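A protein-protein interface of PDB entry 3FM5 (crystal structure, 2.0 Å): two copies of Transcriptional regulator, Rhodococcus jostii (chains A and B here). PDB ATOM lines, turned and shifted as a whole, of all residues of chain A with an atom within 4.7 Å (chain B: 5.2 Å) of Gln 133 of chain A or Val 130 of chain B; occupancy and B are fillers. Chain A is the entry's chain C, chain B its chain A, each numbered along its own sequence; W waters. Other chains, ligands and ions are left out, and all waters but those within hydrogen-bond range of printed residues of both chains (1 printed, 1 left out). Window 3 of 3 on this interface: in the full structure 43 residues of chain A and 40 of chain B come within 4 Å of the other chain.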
ATOM      1  N   THR A 129     -22.306 -21.449   3.626  1.00  0.00           N
ATOM      2  CA  THR A 129     -21.817 -22.069   4.857  1.00  0.00           C
ATOM      3  C   THR A 129     -20.682 -21.271   5.491  1.00  0.00           C
ATOM      4  O   THR A 129     -20.568 -21.213   6.711  1.00  0.00           O
ATOM      5  CB  THR A 129     -21.350 -23.526   4.636  1.00  0.00           C
ATOM      6  OG1 THR A 129     -20.458 -23.582   3.516  1.00  0.00           O
ATOM      7  CG2 THR A 129     -22.539 -24.437   4.376  1.00  0.00           C
ATOM      8  N   VAL A 130     -19.843 -20.667   4.655  1.00  0.00           N
ATOM      9  CA  VAL A 130     -18.738 -19.843   5.134  1.00  0.00           C
ATOM     10  C   VAL A 130     -19.258 -18.545   5.750  1.00  0.00           C
ATOM     11  O   VAL A 130     -18.833 -18.146   6.834  1.00  0.00           O
ATOM     12  CB  VAL A 130     -17.748 -19.519   3.999  1.00  0.00           C
ATOM     13  CG1 VAL A 130     -16.704 -18.515   4.471  1.00  0.00           C
ATOM     14  CG2 VAL A 130     -17.088 -20.795   3.492  1.00  0.00           C
ATOM     15  N   VAL A 131     -20.176 -17.884   5.053  1.00  0.00           N
ATOM     16  CA  VAL A 131     -20.849 -16.729   5.627  1.00  0.00           C
ATOM     17  C   VAL A 131     -21.567 -17.127   6.923  1.00  0.00           C
ATOM     18  O   VAL A 131     -21.439 -16.455   7.949  1.00  0.00           O
ATOM     19  CB  VAL A 131     -21.868 -16.111   4.647  1.00  0.00           C
ATOM     20  CG1 VAL A 131     -22.543 -14.907   5.279  1.00  0.00           C
ATOM     21  CG2 VAL A 131     -21.185 -15.711   3.344  1.00  0.00           C
ATOM     22  N   ASN A 132     -22.320 -18.222   6.874  1.00  0.00           N
ATOM     23  CA  ASN A 132     -23.060 -18.683   8.047  1.00  0.00           C
ATOM     24  C   ASN A 132     -22.161 -18.885   9.253  1.00  0.00           C
ATOM     25  O   ASN A 132     -22.552 -18.603  10.387  1.00  0.00           O
ATOM     26  CB  ASN A 132     -23.792 -19.996   7.751  1.00  0.00           C
ATOM     27  CG  ASN A 132     -25.015 -19.803   6.880  1.00  0.00           C
ATOM     28  OD1 ASN A 132     -25.523 -20.753   6.283  1.00  0.00           O
ATOM     29  ND2 ASN A 132     -25.497 -18.569   6.801  1.00  0.00           N
ATOM     30  N   GLN A 133     -20.964 -19.407   9.018  1.00  0.00           N
ATOM     31  CA  GLN A 133     -20.054 -19.653  10.124  1.00  0.00           C
ATOM     32  C   GLN A 133     -19.560 -18.343  10.708  1.00  0.00           C
ATOM     33  O   GLN A 133     -19.434 -18.211  11.923  1.00  0.00           O
ATOM     34  CB  GLN A 133     -18.875 -20.529   9.716  1.00  0.00           C
ATOM     35  CG  GLN A 133     -18.212 -21.185  10.910  1.00  0.00           C
ATOM     36  CD  GLN A 133     -16.939 -21.911  10.545  1.00  0.00           C
ATOM     37  OE1 GLN A 133     -16.092 -21.377   9.831  1.00  0.00           O
ATOM     38  NE2 GLN A 133     -16.789 -23.132  11.047  1.00  0.00           N
ATOM     39  N   MET A 134     -19.287 -17.373   9.843  1.00  0.00           N
ATOM     40  CA  MET A 134     -18.898 -16.056  10.313  1.00  0.00           C
ATOM     41  C   MET A 134     -20.010 -15.486  11.185  1.00  0.00           C
ATOM     42  O   MET A 134     -19.750 -14.953  12.257  1.00  0.00           O
ATOM     43  CB  MET A 134     -18.621 -15.110   9.147  1.00  0.00           C
ATOM     44  CG  MET A 134     -18.206 -13.721   9.597  1.00  0.00           C
ATOM     45  SD  MET A 134     -17.618 -12.636   8.073  1.00  0.00           S
ATOM     46  CE  MET A 134     -19.333 -12.059   7.399  1.00  0.00           C
ATOM     47  N   ARG A 135     -21.247 -15.604  10.720  1.00  0.00           N
ATOM     48  CA  ARG A 135     -22.390 -15.123  11.484  1.00  0.00           C
ATOM     49  C   ARG A 135     -22.396 -15.770  12.865  1.00  0.00           C
ATOM     50  O   ARG A 135     -22.565 -15.094  13.874  1.00  0.00           O
ATOM     51  CB  ARG A 135     -23.703 -15.431  10.758  1.00  0.00           C
ATOM     52  CG  ARG A 135     -24.938 -15.012  11.531  1.00  0.00           C
ATOM     53  CD  ARG A 135     -26.229 -15.336  10.790  1.00  0.00           C
ATOM     54  NE  ARG A 135     -26.394 -14.509   9.601  1.00  0.00           N
ATOM     55  CZ  ARG A 135     -26.215 -14.949   8.361  1.00  0.00           C
ATOM     56  NH1 ARG A 135     -25.879 -16.212   8.151  1.00  0.00           N
ATOM     57  NH2 ARG A 135     -26.374 -14.128   7.336  1.00  0.00           N
ATOM     58  N   ASP A 136     -22.200 -17.066  12.904  1.00  0.00           N
ATOM     59  CA  ASP A 136     -22.185 -17.797  14.140  1.00  0.00           C
ATOM     60  C   ASP A 136     -21.094 -17.338  15.078  1.00  0.00           C
ATOM     61  O   ASP A 136     -21.321 -17.185  16.241  1.00  0.00           O
ATOM     62  CB  ASP A 136     -22.091 -19.281  13.854  1.00  0.00           C
ATOM     63  CG  ASP A 136     -23.359 -19.825  13.308  1.00  0.00           C
ATOM     64  OD1 ASP A 136     -23.348 -20.916  12.791  1.00  0.00           O
ATOM     65  OD2 ASP A 136     -24.372 -19.158  13.381  1.00  0.00           O
ATOM     66  N   THR A 137     -19.911 -17.097  14.573  1.00  0.00           N
ATOM     67  CA  THR A 137     -18.844 -16.670  15.476  1.00  0.00           C
ATOM     68  C   THR A 137     -19.091 -15.251  15.992  1.00  0.00           C
ATOM     69  O   THR A 137     -18.857 -14.973  17.163  1.00  0.00           O
ATOM     70  CB  THR A 137     -17.405 -16.824  14.895  1.00  0.00           C
ATOM     71  OG1 THR A 137     -16.882 -15.552  14.510  1.00  0.00           O
ATOM     72  CG2 THR A 137     -17.379 -17.773  13.725  1.00  0.00           C
ATOM     73  N   ILE B 126     -13.025 -19.630  20.849  1.00  0.00           N
ATOM     74  CA  ILE B 126     -13.482 -19.915  19.496  1.00  0.00           C
ATOM     75  C   ILE B 126     -12.351 -20.657  18.790  1.00  0.00           C
ATOM     76  O   ILE B 126     -11.216 -20.199  18.805  1.00  0.00           O
ATOM     77  CB  ILE B 126     -13.851 -18.624  18.722  1.00  0.00           C
ATOM     78  CG1 ILE B 126     -14.867 -17.793  19.511  1.00  0.00           C
ATOM     79  CG2 ILE B 126     -14.424 -18.963  17.347  1.00  0.00           C
ATOM     80  CD1 ILE B 126     -15.287 -16.496  18.807  1.00  0.00           C
ATOM     81  N   PRO B 127     -12.642 -21.822  18.191  1.00  0.00           N
ATOM     82  CA  PRO B 127     -11.541 -22.592  17.595  1.00  0.00           C
ATOM     83  C   PRO B 127     -10.745 -21.768  16.582  1.00  0.00           C
ATOM     84  O   PRO B 127     -11.316 -20.956  15.852  1.00  0.00           O
ATOM     85  CB  PRO B 127     -12.258 -23.756  16.903  1.00  0.00           C
ATOM     86  CG  PRO B 127     -13.542 -23.906  17.657  1.00  0.00           C
ATOM     87  CD  PRO B 127     -13.941 -22.495  18.027  1.00  0.00           C
ATOM     88  N   ASP B 128      -9.434 -21.979  16.539  1.00  0.00           N
ATOM     89  CA  ASP B 128      -8.565 -21.166  15.701  1.00  0.00           C
ATOM     90  C   ASP B 128      -8.909 -21.265  14.216  1.00  0.00           C
ATOM     91  O   ASP B 128      -8.861 -20.266  13.502  1.00  0.00           O
ATOM     92  CB  ASP B 128      -7.089 -21.523  15.933  1.00  0.00           C
ATOM     93  CG  ASP B 128      -6.560 -20.984  17.252  1.00  0.00           C
ATOM     94  OD1 ASP B 128      -7.315 -20.282  17.956  1.00  0.00           O
ATOM     95  OD2 ASP B 128      -5.389 -21.260  17.586  1.00  0.00           O
ATOM     96  N   THR B 129      -9.247 -22.464  13.748  1.00  0.00           N
ATOM     97  CA  THR B 129      -9.577 -22.635  12.338  1.00  0.00           C
ATOM     98  C   THR B 129     -10.751 -21.742  11.978  1.00  0.00           C
ATOM     99  O   THR B 129     -10.794 -21.179  10.888  1.00  0.00           O
ATOM    100  CB  THR B 129      -9.933 -24.101  11.973  1.00  0.00           C
ATOM    101  OG1 THR B 129     -11.162 -24.470  12.606  1.00  0.00           O
ATOM    102  CG2 THR B 129      -8.835 -25.050  12.415  1.00  0.00           C
ATOM    103  N   VAL B 130     -11.703 -21.617  12.901  1.00  0.00           N
ATOM    104  CA  VAL B 130     -12.894 -20.816  12.661  1.00  0.00           C
ATOM    105  C   VAL B 130     -12.546 -19.329  12.583  1.00  0.00           C
ATOM    106  O   VAL B 130     -12.990 -18.630  11.675  1.00  0.00           O
ATOM    107  CB  VAL B 130     -13.967 -21.051  13.738  1.00  0.00           C
ATOM    108  CG1 VAL B 130     -15.068 -20.016  13.611  1.00  0.00           C
ATOM    109  CG2 VAL B 130     -14.538 -22.459  13.611  1.00  0.00           C
ATOM    110  N   VAL B 131     -11.738 -18.857  13.528  1.00  0.00           N
ATOM    111  CA  VAL B 131     -11.285 -17.469  13.521  1.00  0.00           C
ATOM    112  C   VAL B 131     -10.409 -17.189  12.304  1.00  0.00           C
ATOM    113  O   VAL B 131     -10.552 -16.154  11.655  1.00  0.00           O
ATOM    114  CB  VAL B 131     -10.500 -17.110  14.804  1.00  0.00           C
ATOM    115  CG1 VAL B 131     -10.074 -15.645  14.776  1.00  0.00           C
ATOM    116  CG2 VAL B 131     -11.338 -17.400  16.044  1.00  0.00           C
ATOM    117  N   ASN B 132      -9.500 -18.114  12.003  1.00  0.00           N
ATOM    118  CA  ASN B 132      -8.600 -17.958  10.866  1.00  0.00           C
ATOM    119  C   ASN B 132      -9.389 -17.845   9.570  1.00  0.00           C
ATOM    120  O   ASN B 132      -9.032 -17.085   8.676  1.00  0.00           O
ATOM    121  CB  ASN B 132      -7.631 -19.140  10.764  1.00  0.00           C
ATOM    122  CG  ASN B 132      -6.490 -19.051  11.754  1.00  0.00           C
ATOM    123  OD1 ASN B 132      -5.898 -20.065  12.127  1.00  0.00           O
ATOM    124  ND2 ASN B 132      -6.171 -17.840  12.181  1.00  0.00           N
ATOM    125  N   GLN B 133     -10.467 -18.612   9.477  1.00  0.00           N
ATOM    126  CA  GLN B 133     -11.296 -18.601   8.286  1.00  0.00           C
ATOM    127  C   GLN B 133     -12.028 -17.273   8.154  1.00  0.00           C
ATOM    128  O   GLN B 133     -12.143 -16.729   7.058  1.00  0.00           O
ATOM    129  CB  GLN B 133     -12.290 -19.761   8.313  1.00  0.00           C
ATOM    130  CG  GLN B 133     -13.213 -19.820   7.112  1.00  0.00           C
ATOM    131  CD  GLN B 133     -13.933 -21.156   7.004  1.00  0.00           C
ATOM    132  OE1 GLN B 133     -14.208 -21.810   8.012  1.00  0.00           O
ATOM    133  NE2 GLN B 133     -14.239 -21.567   5.780  1.00  0.00           N
ATOM    134  N   MET B 134     -12.515 -16.744   9.272  1.00  0.00           N
ATOM    135  CA  MET B 134     -13.192 -15.461   9.231  1.00  0.00           C
ATOM    136  C   MET B 134     -12.249 -14.366   8.752  1.00  0.00           C
ATOM    137  O   MET B 134     -12.646 -13.483   7.987  1.00  0.00           O
ATOM    138  CB  MET B 134     -13.771 -15.079  10.591  1.00  0.00           C
ATOM    139  CG  MET B 134     -14.535 -13.763  10.520  1.00  0.00           C
ATOM    140  SD  MET B 134     -15.434 -13.335  12.176  1.00  0.00           S
ATOM    141  CE  MET B 134     -13.862 -12.805  13.196  1.00  0.00           C
HETATM  142  O   HOH W   1     -15.658 -18.521  10.048  1.00  0.00           O
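Of the 9 printed residues of chain A, 4 touch a printed residue of chain B.
Hydrophobic or aromatic side chains of chain A that line the printed part of chain B: Val 130 and Met 134.
Of the 9 printed residues of chain B, 3 touch a printed residue of chain A.
Printed residues of chain B that touch a printed residue of chain A: Val 130, Gln 133 and Met 134.
Hydrophobic or aromatic side chains of chain B that line the printed part of chain A: Val 130 and Met 134.
Printed residues of chain B within 4 Å of Val 130 of chain A: Gln 133 (3.7 Å).
Of chain B, only Val 130 (3.5 Å) and Gln 133 (2.7 Å) come within 4 Å of Gln 133 of chain A.
Asp 136 of chain A touches none of the printed residues of chain B.
Of the printed residues of chain B, Thr 137 of chain A touches Val 130 (3.2 Å) and Met 134 (3.5 Å).
Of chain A, only Gln 133 and Thr 137 come within 4 Å of Val 130 of chain B.
Printed residues of chain A within 4 Å of Gln 133 of chain B: Val 130 (3.7 Å) and Gln 133 (2.7 Å).
Of the printed residues of chain A, Met 134 of chain B touches Met 134 and Thr 137.
The nearest printed residue of chain A that does not touch Val 130 of chain B is Met 134 of chain A (6.2 Å).
Val 130 of chain A touches Gln 133 of chain B, and with the chains exchanged Gln 133 of chain A touches Val 130 of chain B.
Gln 133 of chain A touches its own counterpart, Gln 133 of chain B.
Met 134 of chain A touches its own counterpart, Met 134 of chain B.
6 positions are printed for both chains.
Of the 6 pairs that touch across the chains among the printed residues, 4 have their exchanged pair printed and touching as well.
Among the printed residues, pairs that only touch across the chains: Thr 137 of chain A with Val 130 of chain B (3.2 Å), Gln 133 of chain A with Val 130 of chain B (3.5 Å), Val 130 of chain A with Gln 133 of chain B (3.7 Å) and Met 134 of chain A with Met 134 of chain B (3.8 Å).
Water W1 bridges the side-chain amide oxygen (OE1) of Gln 133 of chain A (2.9 Å) and the backbone carbonyl oxygen (O) of Val 130 of chain B (3.1 Å).
OE1 of Gln 133 of chain B lies close to OE1 of Gln 133 of chain A, at 2.7 Å.
The side-chain sulfur of Met 134 of chain B lies within hydrogen-bond range of the side-chain hydroxyl of Thr 137 of chain A (3.5 Å).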
